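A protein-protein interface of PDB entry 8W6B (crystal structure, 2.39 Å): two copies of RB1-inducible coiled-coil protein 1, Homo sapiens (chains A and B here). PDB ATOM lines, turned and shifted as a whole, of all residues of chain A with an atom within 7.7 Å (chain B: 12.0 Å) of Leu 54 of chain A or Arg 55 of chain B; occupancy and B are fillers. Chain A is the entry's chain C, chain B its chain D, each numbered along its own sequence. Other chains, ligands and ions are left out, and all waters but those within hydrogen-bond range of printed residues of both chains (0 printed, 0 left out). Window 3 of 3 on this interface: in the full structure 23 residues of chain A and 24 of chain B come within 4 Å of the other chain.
NH2 of Arg 55 of chain B lies within salt-bridge range of OE1 of Glu 50 of chain A (3.0 Å).
The guanidinium group (NH2) of Arg 55 of chain A is in salt-bridge range of the side-chain carboxylate (OE2) of Glu 50 of chain B (2.7 Å).
The backbone carbonyl oxygen (O) of Val 51 of chain B lies close to the guanidinium group (NE) of Arg 55 of chain B, 3.5 Å away.
The guanidinium group of Arg 55 of chain A lies close to the backbone carbonyl oxygen of Val 51 of chain A, at 3.5 Å.
Glu 48 of chain A touches Leu 47 of chain B.
Leu 47 of chain B touches Val 51 of chain A.
Val 51 of chain A touches Glu 50 of chain B.
Val 51 of chain A touches Val 51 of chain B (CG2 to CG1, 3.5 Å).
Leu 54 of chain A touches Arg 55 of chain B.
CD2 of Leu 54 of chain B touches NH2 of Arg 55 of chain A, at 3.3 Å.
Glu 50 of chain A touches one residue of chain B.
Of chain B, only Leu 47, Glu 50 and Val 51 come within 4 Å of Val 51 of chain A.
No residue of chain B comes within 4 Å of Ser 52 of chain A.
Leu 54 of chain A touches one residue of chain B.
No residue of chain B comes within 4 Å of Ser 57 of chain A.
Lys 46 of chain B touches none of the printed residues of chain A.
Printed residues of chain A within 4 Å of Glu 50 of chain B: Val 51 (3.0 Å) and Arg 55 (2.7 Å).
Printed residues of chain A within 4 Å of Val 51 of chain B: Val 51.
Arg 55 of chain B touches just these residues of chain A: Glu 50 and Leu 54.
The nearest residue of chain B that does not touch Leu 54 of chain A is Leu 54 of chain B (4.1 Å).
The nearest residue of chain A that does not touch Arg 55 of chain B is Val 51 of chain A (6.8 Å).
The nearest printed residue of chain A that does not touch Glu 50 of chain B is Ser 52 of chain A (6.3 Å).
Of the 10 printed residues of chain B, 5 touch a printed residue of chain A.
Printed residues of chain B that touch a printed residue of chain A: Leu 47, Glu 50, Val 51, Leu 54 and Arg 55.
Hydrophobic or aromatic side chains of chain B within 4 Å of the printed part of chain A: Leu 47, Val 51 and Leu 54.
Among the printed residues, Asp or Glu carboxylates within 4 Å of a Lys or Arg side-chain nitrogen of the other chain: Glu 50 of chain A with Arg 55 of chain B (3.0 Å) and Arg 55 of chain A with Glu 50 of chain B (2.7 Å).
Glu 50 of chain A touches Arg 55 of chain B, and with the chains exchanged Arg 55 of chain A touches Glu 50 of chain B.
Val 51 of chain A touches Glu 50 of chain B, but with the chains exchanged Glu 50 of chain A does not touch Val 51 of chain B (4.6 Å).
Val 51 of chain B touches its own counterpart, Val 51 of chain A.
Leu 54 of chain A touches Arg 55 of chain B, and with the chains exchanged Arg 55 of chain A touches Leu 54 of chain B.
Of the 8 pairs that touch across the chains among the printed residues, 5 have their exchanged pair printed and touching as well.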
ATOM      1  N   GLU A  48      12.429  -7.559 -14.640  1.00  0.00           N
ATOM      2  CA  GLU A  48      13.826  -7.575 -14.210  1.00  0.00           C
ATOM      3  C   GLU A  48      13.953  -7.986 -12.752  1.00  0.00           C
ATOM      4  O   GLU A  48      14.948  -8.619 -12.372  1.00  0.00           O
ATOM      5  CB  GLU A  48      14.479  -6.206 -14.436  1.00  0.00           C
ATOM      6  CG  GLU A  48      14.717  -5.843 -15.893  1.00  0.00           C
ATOM      7  CD  GLU A  48      14.833  -4.338 -16.098  1.00  0.00           C
ATOM      8  OE1 GLU A  48      15.513  -3.904 -17.056  1.00  0.00           O
ATOM      9  OE2 GLU A  48      14.236  -3.587 -15.294  1.00  0.00           O
ATOM     10  N   GLU A  49      12.953  -7.661 -11.929  1.00  0.00           N
ATOM     11  CA  GLU A  49      13.036  -7.990 -10.510  1.00  0.00           C
ATOM     12  C   GLU A  49      12.940  -9.489 -10.289  1.00  0.00           C
ATOM     13  O   GLU A  49      13.694 -10.048  -9.485  1.00  0.00           O
ATOM     14  CB  GLU A  49      11.947  -7.268  -9.711  1.00  0.00           C
ATOM     15  CG  GLU A  49      11.839  -5.746  -9.923  1.00  0.00           C
ATOM     16  CD  GLU A  49      13.138  -5.072 -10.381  1.00  0.00           C
ATOM     17  OE1 GLU A  49      13.061  -4.048 -11.100  1.00  0.00           O
ATOM     18  OE2 GLU A  49      14.236  -5.547 -10.015  1.00  0.00           O
ATOM     19  N   GLU A  50      12.031 -10.160 -10.999  1.00  0.00           N
ATOM     20  CA  GLU A  50      11.898 -11.605 -10.840  1.00  0.00           C
ATOM     21  C   GLU A  50      13.112 -12.355 -11.382  1.00  0.00           C
ATOM     22  O   GLU A  50      13.386 -13.478 -10.943  1.00  0.00           O
ATOM     23  CB  GLU A  50      10.612 -12.101 -11.510  1.00  0.00           C
ATOM     24  CG  GLU A  50       9.341 -11.470 -10.944  1.00  0.00           C
ATOM     25  CD  GLU A  50       8.212 -12.480 -10.771  1.00  0.00           C
ATOM     26  OE1 GLU A  50       8.052 -13.351 -11.653  1.00  0.00           O
ATOM     27  OE2 GLU A  50       7.488 -12.408  -9.750  1.00  0.00           O
ATOM     28  N   VAL A  51      13.854 -11.749 -12.310  1.00  0.00           N
ATOM     29  CA  VAL A  51      15.141 -12.299 -12.722  1.00  0.00           C
ATOM     30  C   VAL A  51      16.133 -12.244 -11.566  1.00  0.00           C
ATOM     31  O   VAL A  51      16.703 -13.265 -11.164  1.00  0.00           O
ATOM     32  CB  VAL A  51      15.668 -11.548 -13.959  1.00  0.00           C
ATOM     33  CG1 VAL A  51      17.064 -12.028 -14.318  1.00  0.00           C
ATOM     34  CG2 VAL A  51      14.716 -11.741 -15.114  1.00  0.00           C
ATOM     35  N   SER A  52      16.356 -11.046 -11.018  1.00  0.00           N
ATOM     36  CA  SER A  52      17.292 -10.904  -9.909  1.00  0.00           C
ATOM     37  C   SER A  52      16.843 -11.700  -8.690  1.00  0.00           C
ATOM     38  O   SER A  52      17.684 -12.255  -7.972  1.00  0.00           O
ATOM     39  CB  SER A  52      17.463  -9.426  -9.562  1.00  0.00           C
ATOM     40  OG  SER A  52      17.893  -9.259  -8.222  1.00  0.00           O
ATOM     41  N   LYS A  53      15.530 -11.790  -8.453  1.00  0.00           N
ATOM     42  CA  LYS A  53      14.983 -12.495  -7.296  1.00  0.00           C
ATOM     43  C   LYS A  53      14.908 -14.002  -7.472  1.00  0.00           C
ATOM     44  O   LYS A  53      14.472 -14.695  -6.539  1.00  0.00           O
ATOM     45  CB  LYS A  53      13.585 -11.962  -6.941  1.00  0.00           C
ATOM     46  CG  LYS A  53      13.565 -10.582  -6.284  1.00  0.00           C
ATOM     47  CD  LYS A  53      14.681 -10.418  -5.243  1.00  0.00           C
ATOM     48  CE  LYS A  53      15.863  -9.643  -5.833  1.00  0.00           C
ATOM     49  NZ  LYS A  53      17.125  -9.794  -5.050  1.00  0.00           N
ATOM     50  N   LEU A  54      15.312 -14.525  -8.632  1.00  0.00           N
ATOM     51  CA  LEU A  54      15.328 -15.964  -8.831  1.00  0.00           C
ATOM     52  C   LEU A  54      16.728 -16.529  -9.035  1.00  0.00           C
ATOM     53  O   LEU A  54      16.909 -17.750  -8.896  1.00  0.00           O
ATOM     54  CB  LEU A  54      14.417 -16.367  -9.996  1.00  0.00           C
ATOM     55  CG  LEU A  54      13.024 -16.822  -9.506  1.00  0.00           C
ATOM     56  CD1 LEU A  54      12.279 -15.731  -8.729  1.00  0.00           C
ATOM     57  CD2 LEU A  54      12.170 -17.428 -10.612  1.00  0.00           C
ATOM     58  N   ARG A  55      17.728 -15.681  -9.336  1.00  0.00           N
ATOM     59  CA  ARG A  55      19.107 -16.066  -9.036  1.00  0.00           C
ATOM     60  C   ARG A  55      19.464 -15.830  -7.573  1.00  0.00           C
ATOM     61  O   ARG A  55      20.412 -16.449  -7.077  1.00  0.00           O
ATOM     62  CB  ARG A  55      20.111 -15.342  -9.939  1.00  0.00           C
ATOM     63  CG  ARG A  55      19.874 -13.860 -10.194  1.00  0.00           C
ATOM     64  CD  ARG A  55      20.257 -13.512 -11.633  1.00  0.00           C
ATOM     65  NE  ARG A  55      19.641 -14.443 -12.576  1.00  0.00           N
ATOM     66  CZ  ARG A  55      20.059 -14.663 -13.824  1.00  0.00           C
ATOM     67  NH1 ARG A  55      21.115 -14.017 -14.308  1.00  0.00           N
ATOM     68  NH2 ARG A  55      19.416 -15.539 -14.595  1.00  0.00           N
ATOM     69  N   SER A  56      18.708 -14.958  -6.869  1.00  0.00           N
ATOM     70  CA  SER A  56      18.657 -14.883  -5.407  1.00  0.00           C
ATOM     71  C   SER A  56      17.975 -16.138  -4.775  1.00  0.00           C
ATOM     72  O   SER A  56      17.821 -16.201  -3.539  1.00  0.00           O
ATOM     73  CB  SER A  56      17.913 -13.622  -4.954  1.00  0.00           C
ATOM     74  OG  SER A  56      18.668 -12.443  -5.184  1.00  0.00           O
ATOM     75  N   SER A  57      17.580 -17.077  -5.639  1.00  0.00           N
ATOM     76  CA  SER A  57      16.845 -18.283  -5.260  1.00  0.00           C
ATOM     77  C   SER A  57      17.569 -19.553  -5.721  1.00  0.00           C
ATOM     78  O   SER A  57      18.173 -20.279  -4.921  1.00  0.00           O
ATOM     79  CB  SER A  57      15.429 -18.254  -5.856  1.00  0.00           C
ATOM     80  OG  SER A  57      14.676 -17.153  -5.372  1.00  0.00           O
ATOM     81  OXT SER A  57      17.561 -19.885  -6.912  1.00  0.00           O
ATOM     82  N   LYS B  46      12.279 -11.131 -24.351  1.00  0.00           N
ATOM     83  CA  LYS B  46      13.469 -11.857 -23.932  1.00  0.00           C
ATOM     84  C   LYS B  46      13.615 -11.944 -22.403  1.00  0.00           C
ATOM     85  O   LYS B  46      14.334 -12.823 -21.910  1.00  0.00           O
ATOM     86  CB  LYS B  46      14.706 -11.209 -24.564  1.00  0.00           C
ATOM     87  CG  LYS B  46      16.001 -11.965 -24.320  1.00  0.00           C
ATOM     88  CD  LYS B  46      17.235 -11.194 -24.767  1.00  0.00           C
ATOM     89  CE  LYS B  46      18.374 -11.317 -23.749  1.00  0.00           C
ATOM     90  NZ  LYS B  46      19.424 -10.295 -24.049  1.00  0.00           N
ATOM     91  N   LEU B  47      12.949 -11.076 -21.627  1.00  0.00           N
ATOM     92  CA  LEU B  47      13.044 -11.209 -20.171  1.00  0.00           C
ATOM     93  C   LEU B  47      12.128 -12.311 -19.655  1.00  0.00           C
ATOM     94  O   LEU B  47      12.514 -13.066 -18.758  1.00  0.00           O
ATOM     95  CB  LEU B  47      12.734  -9.882 -19.481  1.00  0.00           C
ATOM     96  CG  LEU B  47      13.956  -9.027 -19.178  1.00  0.00           C
ATOM     97  CD1 LEU B  47      13.613  -7.557 -19.129  1.00  0.00           C
ATOM     98  CD2 LEU B  47      14.548  -9.466 -17.876  1.00  0.00           C
ATOM     99  N   GLU B  48      10.916 -12.422 -20.209  1.00  0.00           N
ATOM    100  CA  GLU B  48      10.075 -13.567 -19.886  1.00  0.00           C
ATOM    101  C   GLU B  48      10.759 -14.870 -20.285  1.00  0.00           C
ATOM    102  O   GLU B  48      10.571 -15.909 -19.634  1.00  0.00           O
ATOM    103  CB  GLU B  48       8.719 -13.431 -20.576  1.00  0.00           C
ATOM    104  CG  GLU B  48       7.950 -12.179 -20.201  1.00  0.00           C
ATOM    105  CD  GLU B  48       6.733 -11.973 -21.078  1.00  0.00           C
ATOM    106  OE1 GLU B  48       5.783 -11.280 -20.656  1.00  0.00           O
ATOM    107  OE2 GLU B  48       6.720 -12.523 -22.193  1.00  0.00           O
ATOM    108  N   GLU B  49      11.568 -14.818 -21.342  1.00  0.00           N
ATOM    109  CA  GLU B  49      12.385 -15.953 -21.742  1.00  0.00           C
ATOM    110  C   GLU B  49      13.322 -16.385 -20.617  1.00  0.00           C
ATOM    111  O   GLU B  49      13.527 -17.587 -20.391  1.00  0.00           O
ATOM    112  CB  GLU B  49      13.167 -15.570 -23.000  1.00  0.00           C
ATOM    113  CG  GLU B  49      13.948 -16.682 -23.658  1.00  0.00           C
ATOM    114  CD  GLU B  49      14.067 -16.490 -25.167  1.00  0.00           C
ATOM    115  OE1 GLU B  49      13.469 -15.534 -25.707  1.00  0.00           O
ATOM    116  OE2 GLU B  49      14.762 -17.300 -25.817  1.00  0.00           O
ATOM    117  N   GLU B  50      13.896 -15.422 -19.895  1.00  0.00           N
ATOM    118  CA  GLU B  50      14.838 -15.765 -18.839  1.00  0.00           C
ATOM    119  C   GLU B  50      14.127 -16.228 -17.575  1.00  0.00           C
ATOM    120  O   GLU B  50      14.651 -17.083 -16.853  1.00  0.00           O
ATOM    121  CB  GLU B  50      15.746 -14.572 -18.534  1.00  0.00           C
ATOM    122  CG  GLU B  50      16.962 -14.924 -17.693  1.00  0.00           C
ATOM    123  CD  GLU B  50      17.817 -13.713 -17.363  1.00  0.00           C
ATOM    124  OE1 GLU B  50      17.784 -12.731 -18.134  1.00  0.00           O
ATOM    125  OE2 GLU B  50      18.531 -13.744 -16.337  1.00  0.00           O
ATOM    126  N   VAL B  51      12.934 -15.699 -17.300  1.00  0.00           N
ATOM    127  CA  VAL B  51      12.237 -16.076 -16.075  1.00  0.00           C
ATOM    128  C   VAL B  51      11.632 -17.468 -16.198  1.00  0.00           C
ATOM    129  O   VAL B  51      11.623 -18.235 -15.229  1.00  0.00           O
ATOM    130  CB  VAL B  51      11.177 -15.022 -15.691  1.00  0.00           C
ATOM    131  CG1 VAL B  51      11.794 -13.631 -15.637  1.00  0.00           C
ATOM    132  CG2 VAL B  51       9.969 -15.059 -16.630  1.00  0.00           C
ATOM    133  N   SER B  52      11.129 -17.831 -17.380  1.00  0.00           N
ATOM    134  CA  SER B  52      10.558 -19.163 -17.557  1.00  0.00           C
ATOM    135  C   SER B  52      11.624 -20.239 -17.730  1.00  0.00           C
ATOM    136  O   SER B  52      11.354 -21.410 -17.433  1.00  0.00           O
ATOM    137  CB  SER B  52       9.586 -19.162 -18.740  1.00  0.00           C
ATOM    138  OG  SER B  52      10.234 -19.552 -19.930  1.00  0.00           O
ATOM    139  N   LYS B  53      12.826 -19.863 -18.184  1.00  0.00           N
ATOM    140  CA  LYS B  53      13.954 -20.782 -18.236  1.00  0.00           C
ATOM    141  C   LYS B  53      14.687 -20.876 -16.902  1.00  0.00           C
ATOM    142  O   LYS B  53      15.421 -21.850 -16.675  1.00  0.00           O
ATOM    143  CB  LYS B  53      14.927 -20.367 -19.346  1.00  0.00           C
ATOM    144  CG  LYS B  53      16.020 -21.394 -19.629  1.00  0.00           C
ATOM    145  CD  LYS B  53      17.166 -20.828 -20.460  1.00  0.00           C
ATOM    146  CE  LYS B  53      16.824 -20.839 -21.950  1.00  0.00           C
ATOM    147  NZ  LYS B  53      16.179 -19.564 -22.387  1.00  0.00           N
ATOM    148  N   LEU B  54      14.491 -19.904 -16.005  1.00  0.00           N
ATOM    149  CA  LEU B  54      14.958 -20.020 -14.627  1.00  0.00           C
ATOM    150  C   LEU B  54      14.017 -20.848 -13.754  1.00  0.00           C
ATOM    151  O   LEU B  54      14.308 -21.038 -12.568  1.00  0.00           O
ATOM    152  CB  LEU B  54      15.149 -18.629 -14.013  1.00  0.00           C
ATOM    153  CG  LEU B  54      16.550 -18.001 -13.960  1.00  0.00           C
ATOM    154  CD1 LEU B  54      17.324 -18.176 -15.265  1.00  0.00           C
ATOM    155  CD2 LEU B  54      16.436 -16.518 -13.618  1.00  0.00           C
ATOM    156  N   ARG B  55      12.915 -21.352 -14.306  1.00  0.00           N
ATOM    157  CA  ARG B  55      12.007 -22.226 -13.562  1.00  0.00           C
ATOM    158  C   ARG B  55      11.989 -23.660 -14.108  1.00  0.00           C
ATOM    159  O   ARG B  55      12.818 -24.038 -14.938  1.00  0.00           O
ATOM    160  CB  ARG B  55      10.588 -21.650 -13.574  1.00  0.00           C
ATOM    161  CG  ARG B  55      10.374 -20.537 -12.573  1.00  0.00           C
ATOM    162  CD  ARG B  55       9.600 -19.386 -13.181  1.00  0.00           C
ATOM    163  NE  ARG B  55       9.684 -18.176 -12.365  1.00  0.00           N
ATOM    164  CZ  ARG B  55       8.665 -17.350 -12.125  1.00  0.00           C
ATOM    165  NH1 ARG B  55       7.468 -17.598 -12.646  1.00  0.00           N
ATOM    166  NH2 ARG B  55       8.846 -16.265 -11.371  1.00  0.00           N
